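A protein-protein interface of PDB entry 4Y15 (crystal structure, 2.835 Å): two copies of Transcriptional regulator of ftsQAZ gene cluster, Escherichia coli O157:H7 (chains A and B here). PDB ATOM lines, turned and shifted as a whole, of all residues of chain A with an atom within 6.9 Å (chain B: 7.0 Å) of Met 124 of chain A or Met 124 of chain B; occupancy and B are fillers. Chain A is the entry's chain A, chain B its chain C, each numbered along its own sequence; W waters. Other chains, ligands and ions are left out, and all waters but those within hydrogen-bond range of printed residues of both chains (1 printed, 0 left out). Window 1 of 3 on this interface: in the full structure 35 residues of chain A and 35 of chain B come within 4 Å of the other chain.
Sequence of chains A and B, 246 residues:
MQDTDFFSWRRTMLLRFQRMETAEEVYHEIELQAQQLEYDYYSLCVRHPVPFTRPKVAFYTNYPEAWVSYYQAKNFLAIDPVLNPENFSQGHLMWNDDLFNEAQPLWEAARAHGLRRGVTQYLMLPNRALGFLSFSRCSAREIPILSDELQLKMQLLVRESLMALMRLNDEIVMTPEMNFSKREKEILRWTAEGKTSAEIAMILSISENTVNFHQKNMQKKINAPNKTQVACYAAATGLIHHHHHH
The side-chain sulfur (SD) of Met 124 of chain A sits at hydrogen-bond distance from the guanidinium group (NH1) of Arg 128 of chain B (3.2 Å).
A ring nitrogen (NE2) of His 241 of chain A lies close to the guanidinium group (NH1) of Arg 128 of chain A (3.1 Å).
The backbone carbonyl oxygen of Pro 126 of chain A sits at hydrogen-bond distance from the guanidinium group of Arg 128 of chain A (2.6 Å).
NH1 of Arg 128 of chain B lies within hydrogen-bond range of O of Pro 126 of chain B, at 2.9 Å.
Met 124 of chain A touches Met 124 of chain B.
Met 124 of chain A touches Leu 125 of chain B (CE to O, 3.4 Å).
Met 124 of chain B touches Arg 128 of chain A.
Met 124 of chain A touches just these residues of chain B: Met 124, Leu 125 and Arg 128.
Pro 126 of chain A touches none of the printed residues of chain B.
Printed residues of chain B within 4 Å of Arg 128 of chain A: Met 124.
Of chain A, only Met 124 and Arg 128 come within 4 Å of Met 124 of chain B.
Of the printed residues of chain A, Leu 125 of chain B touches Met 124 (3.4 Å).
Of the printed residues of chain A, Arg 128 of chain B touches Met 124.
The nearest residue of chain B that does not touch Met 124 of chain A is Pro 126 of chain B (4.5 Å).
The nearest printed residue of chain A that does not touch Arg 128 of chain B is Arg 128 of chain A (4.3 Å).
Hydrophobic or aromatic side chains of chain A within 4 Å of the printed part of chain B: Met 124.
Along chain A the printed residues that touch a printed residue of chain B span positions 124 to 128.
Hydrophobic or aromatic side chains of chain B that line the printed part of chain A: Met 124.
Among the printed residues, no Asp or Glu carboxylate lies within 4 Å of a Lys or Arg side-chain nitrogen of the other chain.
Met 124 of chain A touches its own counterpart, Met 124 of chain B.
Met 124 of chain A touches Leu 125 of chain B, but with the chains exchanged Leu 125 of chain A does not touch Met 124 of chain B (4.5 Å).
Met 124 of chain A touches Arg 128 of chain B, and with the chains exchanged Arg 128 of chain A touches Met 124 of chain B.
Of the 4 pairs that touch across the chains among the printed residues, 3 have their exchanged pair printed and touching as well.
Water W1 lies within hydrogen-bond range of the backbone carbonyl oxygen (O) of Ala 236 of chain B (2.7 Å), a ring nitrogen (NE2) of His 241 of chain A (3.0 Å) and the guanidinium group (NE) of Arg 128 of chain A (3.0 Å).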
ATOM      1  N   TYR A 122      21.876  36.618 -13.392  1.00  0.00           N
ATOM      2  CA  TYR A 122      21.387  35.997 -14.624  1.00  0.00           C
ATOM      3  C   TYR A 122      20.380  34.871 -14.385  1.00  0.00           C
ATOM      4  O   TYR A 122      20.334  34.283 -13.302  1.00  0.00           O
ATOM      5  CB  TYR A 122      22.569  35.459 -15.436  1.00  0.00           C
ATOM      6  CG  TYR A 122      22.783  33.967 -15.300  1.00  0.00           C
ATOM      7  CD1 TYR A 122      22.246  33.080 -16.227  1.00  0.00           C
ATOM      8  CD2 TYR A 122      23.521  33.446 -14.248  1.00  0.00           C
ATOM      9  CE1 TYR A 122      22.439  31.717 -16.106  1.00  0.00           C
ATOM     10  CE2 TYR A 122      23.720  32.083 -14.119  1.00  0.00           C
ATOM     11  CZ  TYR A 122      23.177  31.223 -15.050  1.00  0.00           C
ATOM     12  OH  TYR A 122      23.371  29.866 -14.925  1.00  0.00           O
ATOM     13  N   LEU A 123      19.572  34.585 -15.408  1.00  0.00           N
ATOM     14  CA  LEU A 123      18.703  33.407 -15.414  1.00  0.00           C
ATOM     15  C   LEU A 123      18.459  32.917 -16.841  1.00  0.00           C
ATOM     16  O   LEU A 123      18.869  33.554 -17.813  1.00  0.00           O
ATOM     17  CB  LEU A 123      17.353  33.694 -14.744  1.00  0.00           C
ATOM     18  CG  LEU A 123      16.239  34.325 -15.589  1.00  0.00           C
ATOM     19  CD1 LEU A 123      14.944  34.392 -14.794  1.00  0.00           C
ATOM     20  CD2 LEU A 123      16.632  35.702 -16.077  1.00  0.00           C
ATOM     21  N   MET A 124      17.801  31.766 -16.949  1.00  0.00           N
ATOM     22  CA  MET A 124      17.392  31.224 -18.235  1.00  0.00           C
ATOM     23  C   MET A 124      15.909  31.502 -18.436  1.00  0.00           C
ATOM     24  O   MET A 124      15.115  31.339 -17.511  1.00  0.00           O
ATOM     25  CB  MET A 124      17.646  29.722 -18.310  1.00  0.00           C
ATOM     26  CG  MET A 124      17.289  29.122 -19.657  1.00  0.00           C
ATOM     27  SD  MET A 124      17.708  27.379 -19.785  1.00  0.00           S
ATOM     28  CE  MET A 124      16.680  26.708 -18.481  1.00  0.00           C
ATOM     29  N   LEU A 125      15.542  31.937 -19.637  1.00  0.00           N
ATOM     30  CA  LEU A 125      14.155  32.265 -19.939  1.00  0.00           C
ATOM     31  C   LEU A 125      13.444  31.046 -20.535  1.00  0.00           C
ATOM     32  O   LEU A 125      14.100  30.084 -20.933  1.00  0.00           O
ATOM     33  CB  LEU A 125      14.096  33.454 -20.892  1.00  0.00           C
ATOM     34  CG  LEU A 125      14.709  34.729 -20.307  1.00  0.00           C
ATOM     35  CD1 LEU A 125      14.840  35.788 -21.388  1.00  0.00           C
ATOM     36  CD2 LEU A 125      13.928  35.257 -19.107  1.00  0.00           C
ATOM     37  N   PRO A 126      12.103  31.085 -20.607  1.00  0.00           N
ATOM     38  CA  PRO A 126      11.346  29.951 -21.161  1.00  0.00           C
ATOM     39  C   PRO A 126      11.727  29.586 -22.600  1.00  0.00           C
ATOM     40  O   PRO A 126      11.513  28.440 -22.997  1.00  0.00           O
ATOM     41  CB  PRO A 126       9.894  30.434 -21.088  1.00  0.00           C
ATOM     42  CG  PRO A 126       9.879  31.420 -19.981  1.00  0.00           C
ATOM     43  CD  PRO A 126      11.210  32.107 -20.032  1.00  0.00           C
ATOM     44  N   ASN A 127      12.269  30.534 -23.362  1.00  0.00           N
ATOM     45  CA  ASN A 127      12.791  30.245 -24.699  1.00  0.00           C
ATOM     46  C   ASN A 127      14.269  29.839 -24.678  1.00  0.00           C
ATOM     47  O   ASN A 127      14.944  29.856 -25.708  1.00  0.00           O
ATOM     48  CB  ASN A 127      12.606  31.458 -25.612  1.00  0.00           C
ATOM     49  CG  ASN A 127      13.267  32.707 -25.065  1.00  0.00           C
ATOM     50  OD1 ASN A 127      14.049  32.646 -24.116  1.00  0.00           O
ATOM     51  ND2 ASN A 127      12.964  33.849 -25.668  1.00  0.00           N
ATOM     52  N   ARG A 128      14.748  29.470 -23.492  1.00  0.00           N
ATOM     53  CA  ARG A 128      16.124  29.016 -23.261  1.00  0.00           C
ATOM     54  C   ARG A 128      17.143  30.135 -23.462  1.00  0.00           C
ATOM     55  O   ARG A 128      18.345  29.876 -23.496  1.00  0.00           O
ATOM     56  CB  ARG A 128      16.519  27.850 -24.176  1.00  0.00           C
ATOM     57  CG  ARG A 128      15.426  26.888 -24.617  1.00  0.00           C
ATOM     58  CD  ARG A 128      14.392  26.595 -23.573  1.00  0.00           C
ATOM     59  NE  ARG A 128      13.760  25.303 -23.824  1.00  0.00           N
ATOM     60  CZ  ARG A 128      12.525  24.977 -23.456  1.00  0.00           C
ATOM     61  NH1 ARG A 128      12.066  23.766 -23.721  1.00  0.00           N
ATOM     62  NH2 ARG A 128      11.742  25.857 -22.844  1.00  0.00           N
ATOM     63  N   ALA A 129      16.674  31.371 -23.600  1.00  0.00           N
ATOM     64  CA  ALA A 129      17.582  32.507 -23.717  1.00  0.00           C
ATOM     65  C   ALA A 129      18.137  32.879 -22.347  1.00  0.00           C
ATOM     66  O   ALA A 129      17.422  32.843 -21.343  1.00  0.00           O
ATOM     67  CB  ALA A 129      16.875  33.696 -24.341  1.00  0.00           C
ATOM     68  N   LEU A 130      19.416  33.240 -22.321  1.00  0.00           N
ATOM     69  CA  LEU A 130      20.079  33.637 -21.088  1.00  0.00           C
ATOM     70  C   LEU A 130      20.042  35.152 -20.940  1.00  0.00           C
ATOM     71  O   LEU A 130      20.524  35.873 -21.808  1.00  0.00           O
ATOM     72  CB  LEU A 130      21.526  33.143 -21.080  1.00  0.00           C
ATOM     73  CG  LEU A 130      21.729  31.630 -20.973  1.00  0.00           C
ATOM     74  CD1 LEU A 130      23.204  31.284 -21.114  1.00  0.00           C
ATOM     75  CD2 LEU A 130      21.166  31.083 -19.668  1.00  0.00           C
ATOM     76  N   GLY A 131      19.482  35.621 -19.829  1.00  0.00           N
ATOM     77  CA  GLY A 131      19.370  37.044 -19.558  1.00  0.00           C
ATOM     78  C   GLY A 131      20.345  37.476 -18.480  1.00  0.00           C
ATOM     79  O   GLY A 131      20.477  36.802 -17.464  1.00  0.00           O
ATOM     80  N   MET A 163      10.528  39.009 -18.229  1.00  0.00           N
ATOM     81  CA  MET A 163       9.226  38.393 -18.450  1.00  0.00           C
ATOM     82  C   MET A 163       8.268  39.465 -18.954  1.00  0.00           C
ATOM     83  O   MET A 163       7.451  39.219 -19.843  1.00  0.00           O
ATOM     84  CB  MET A 163       8.693  37.741 -17.171  1.00  0.00           C
ATOM     85  CG  MET A 163       9.485  36.514 -16.706  1.00  0.00           C
ATOM     86  SD  MET A 163       9.739  35.236 -17.957  1.00  0.00           S
ATOM     87  CE  MET A 163       8.059  34.706 -18.267  1.00  0.00           C
ATOM     88  N   GLY A 238      12.519  25.519 -27.510  1.00  0.00           N
ATOM     89  CA  GLY A 238      11.404  24.991 -26.743  1.00  0.00           C
ATOM     90  C   GLY A 238      10.057  25.233 -27.403  1.00  0.00           C
ATOM     91  O   GLY A 238       9.011  25.071 -26.774  1.00  0.00           O
ATOM     92  N   HIS A 241       8.032  21.958 -26.883  1.00  0.00           N
ATOM     93  CA  HIS A 241       7.595  21.542 -25.552  1.00  0.00           C
ATOM     94  C   HIS A 241       7.417  22.716 -24.590  1.00  0.00           C
ATOM     95  O   HIS A 241       7.804  22.657 -23.422  1.00  0.00           O
ATOM     96  CB  HIS A 241       8.597  20.512 -25.024  1.00  0.00           C
ATOM     97  CG  HIS A 241      10.007  20.785 -25.438  1.00  0.00           C
ATOM     98  ND1 HIS A 241      10.442  20.603 -26.737  1.00  0.00           N
ATOM     99  CD2 HIS A 241      11.089  21.205 -24.741  1.00  0.00           C
ATOM    100  CE1 HIS A 241      11.719  20.915 -26.822  1.00  0.00           C
ATOM    101  NE2 HIS A 241      12.140  21.283 -25.622  1.00  0.00           N
ATOM    102  N   TYR B 122       6.946  25.489  -9.193  1.00  0.00           N
ATOM    103  CA  TYR B 122       7.657  24.872 -10.306  1.00  0.00           C
ATOM    104  C   TYR B 122       8.780  25.764 -10.806  1.00  0.00           C
ATOM    105  O   TYR B 122       8.754  26.978 -10.621  1.00  0.00           O
ATOM    106  CB  TYR B 122       6.702  24.566 -11.467  1.00  0.00           C
ATOM    107  CG  TYR B 122       6.823  25.546 -12.618  1.00  0.00           C
ATOM    108  CD1 TYR B 122       7.713  25.322 -13.663  1.00  0.00           C
ATOM    109  CD2 TYR B 122       6.053  26.701 -12.653  1.00  0.00           C
ATOM    110  CE1 TYR B 122       7.833  26.221 -14.706  1.00  0.00           C
ATOM    111  CE2 TYR B 122       6.163  27.603 -13.692  1.00  0.00           C
ATOM    112  CZ  TYR B 122       7.054  27.359 -14.716  1.00  0.00           C
ATOM    113  OH  TYR B 122       7.162  28.258 -15.753  1.00  0.00           O
ATOM    114  N   LEU B 123       9.765  25.144 -11.440  1.00  0.00           N
ATOM    115  CA  LEU B 123      10.784  25.874 -12.173  1.00  0.00           C
ATOM    116  C   LEU B 123      11.385  25.027 -13.292  1.00  0.00           C
ATOM    117  O   LEU B 123      11.141  23.823 -13.371  1.00  0.00           O
ATOM    118  CB  LEU B 123      11.851  26.378 -11.201  1.00  0.00           C
ATOM    119  CG  LEU B 123      12.941  25.451 -10.660  1.00  0.00           C
ATOM    120  CD1 LEU B 123      14.076  25.154 -11.630  1.00  0.00           C
ATOM    121  CD2 LEU B 123      13.485  26.084  -9.400  1.00  0.00           C
ATOM    122  N   MET B 124      12.176  25.667 -14.148  1.00  0.00           N
ATOM    123  CA  MET B 124      12.856  24.982 -15.240  1.00  0.00           C
ATOM    124  C   MET B 124      14.336  24.739 -14.946  1.00  0.00           C
ATOM    125  O   MET B 124      15.046  25.637 -14.498  1.00  0.00           O
ATOM    126  CB  MET B 124      12.710  25.796 -16.523  1.00  0.00           C
ATOM    127  CG  MET B 124      13.350  25.154 -17.726  1.00  0.00           C
ATOM    128  SD  MET B 124      13.001  26.071 -19.224  1.00  0.00           S
ATOM    129  CE  MET B 124      13.904  25.079 -20.392  1.00  0.00           C
ATOM    130  N   LEU B 125      14.793  23.524 -15.231  1.00  0.00           N
ATOM    131  CA  LEU B 125      16.166  23.117 -14.956  1.00  0.00           C
ATOM    132  C   LEU B 125      17.092  23.351 -16.151  1.00  0.00           C
ATOM    133  O   LEU B 125      16.623  23.567 -17.268  1.00  0.00           O
ATOM    134  CB  LEU B 125      16.193  21.637 -14.571  1.00  0.00           C
ATOM    135  CG  LEU B 125      15.463  21.254 -13.283  1.00  0.00           C
ATOM    136  CD1 LEU B 125      15.324  19.748 -13.200  1.00  0.00           C
ATOM    137  CD2 LEU B 125      16.198  21.782 -12.063  1.00  0.00           C
ATOM    138  N   PRO B 126      18.416  23.303 -15.918  1.00  0.00           N
ATOM    139  CA  PRO B 126      19.402  23.485 -16.992  1.00  0.00           C
ATOM    140  C   PRO B 126      19.306  22.461 -18.126  1.00  0.00           C
ATOM    141  O   PRO B 126      19.738  22.770 -19.236  1.00  0.00           O
ATOM    142  CB  PRO B 126      20.742  23.352 -16.259  1.00  0.00           C
ATOM    143  CG  PRO B 126      20.449  23.760 -14.869  1.00  0.00           C
ATOM    144  CD  PRO B 126      19.055  23.295 -14.589  1.00  0.00           C
ATOM    145  N   ASN B 127      18.769  21.272 -17.859  1.00  0.00           N
ATOM    146  CA  ASN B 127      18.520  20.296 -18.924  1.00  0.00           C
ATOM    147  C   ASN B 127      17.128  20.475 -19.538  1.00  0.00           C
ATOM    148  O   ASN B 127      16.608  19.582 -20.203  1.00  0.00           O
ATOM    149  CB  ASN B 127      18.689  18.864 -18.404  1.00  0.00           C
ATOM    150  CG  ASN B 127      17.786  18.551 -17.226  1.00  0.00           C
ATOM    151  OD1 ASN B 127      16.874  19.312 -16.900  1.00  0.00           O
ATOM    152  ND2 ASN B 127      18.023  17.408 -16.595  1.00  0.00           N
ATOM    153  N   ARG B 128      16.542  21.643 -19.292  1.00  0.00           N
ATOM    154  CA  ARG B 128      15.242  22.040 -19.833  1.00  0.00           C
ATOM    155  C   ARG B 128      14.047  21.235 -19.316  1.00  0.00           C
ATOM    156  O   ARG B 128      12.934  21.393 -19.822  1.00  0.00           O
ATOM    157  CB  ARG B 128      15.238  21.959 -21.365  1.00  0.00           C
ATOM    158  CG  ARG B 128      16.534  22.314 -22.089  1.00  0.00           C
ATOM    159  CD  ARG B 128      17.262  23.515 -21.529  1.00  0.00           C
ATOM    160  NE  ARG B 128      18.139  24.090 -22.548  1.00  0.00           N
ATOM    161  CZ  ARG B 128      19.229  24.811 -22.300  1.00  0.00           C
ATOM    162  NH1 ARG B 128      19.602  25.069 -21.053  1.00  0.00           N
ATOM    163  NH2 ARG B 128      19.945  25.285 -23.309  1.00  0.00           N
ATOM    164  N   ALA B 129      14.259  20.380 -18.322  1.00  0.00           N
ATOM    165  CA  ALA B 129      13.149  19.663 -17.706  1.00  0.00           C
ATOM    166  C   ALA B 129      12.422  20.563 -16.707  1.00  0.00           C
ATOM    167  O   ALA B 129      13.053  21.337 -15.991  1.00  0.00           O
ATOM    168  CB  ALA B 129      13.642  18.400 -17.025  1.00  0.00           C
ATOM    169  N   LEU B 130      11.096  20.461 -16.665  1.00  0.00           N
ATOM    170  CA  LEU B 130      10.291  21.229 -15.719  1.00  0.00           C
ATOM    171  C   LEU B 130      10.006  20.419 -14.464  1.00  0.00           C
ATOM    172  O   LEU B 130       9.486  19.307 -14.539  1.00  0.00           O
ATOM    173  CB  LEU B 130       8.974  21.685 -16.350  1.00  0.00           C
ATOM    174  CG  LEU B 130       9.028  22.822 -17.375  1.00  0.00           C
ATOM    175  CD1 LEU B 130      10.022  22.566 -18.496  1.00  0.00           C
ATOM    176  CD2 LEU B 130       7.633  23.061 -17.931  1.00  0.00           C
ATOM    177  N   GLY B 131      10.355  20.989 -13.315  1.00  0.00           N
ATOM    178  CA  GLY B 131      10.158  20.340 -12.031  1.00  0.00           C
ATOM    179  C   GLY B 131       9.014  20.963 -11.256  1.00  0.00           C
ATOM    180  O   GLY B 131       8.897  22.185 -11.197  1.00  0.00           O
ATOM    181  N   VAL B 158      12.144  23.695  -4.285  1.00  0.00           N
ATOM    182  CA  VAL B 158      12.079  23.142  -5.641  1.00  0.00           C
ATOM    183  C   VAL B 158      13.437  23.104  -6.322  1.00  0.00           C
ATOM    184  O   VAL B 158      13.827  22.083  -6.886  1.00  0.00           O
ATOM    185  CB  VAL B 158      11.117  23.949  -6.549  1.00  0.00           C
ATOM    186  CG1 VAL B 158      11.145  23.443  -7.991  1.00  0.00           C
ATOM    187  CG2 VAL B 158       9.723  23.933  -5.995  1.00  0.00           C
ATOM    188  N   MET B 163      18.357  20.319  -8.041  1.00  0.00           N
ATOM    189  CA  MET B 163      19.770  20.565  -8.309  1.00  0.00           C
ATOM    190  C   MET B 163      20.624  19.498  -7.636  1.00  0.00           C
ATOM    191  O   MET B 163      21.590  19.003  -8.220  1.00  0.00           O
ATOM    192  CB  MET B 163      20.195  21.953  -7.819  1.00  0.00           C
ATOM    193  CG  MET B 163      19.670  23.130  -8.633  1.00  0.00           C
ATOM    194  SD  MET B 163      20.051  23.002 -10.389  1.00  0.00           S
ATOM    195  CE  MET B 163      20.152  24.736 -10.821  1.00  0.00           C
ATOM    196  N   ALA B 236      17.654  20.067 -27.667  1.00  0.00           N
ATOM    197  CA  ALA B 236      16.512  20.156 -26.769  1.00  0.00           C
ATOM    198  C   ALA B 236      16.948  20.189 -25.311  1.00  0.00           C
ATOM    199  O   ALA B 236      16.201  20.649 -24.454  1.00  0.00           O
ATOM    200  CB  ALA B 236      15.565  18.996 -27.001  1.00  0.00           C
HETATM  201  O   HOH W   1      14.680  22.757 -25.169  1.00  0.00           O
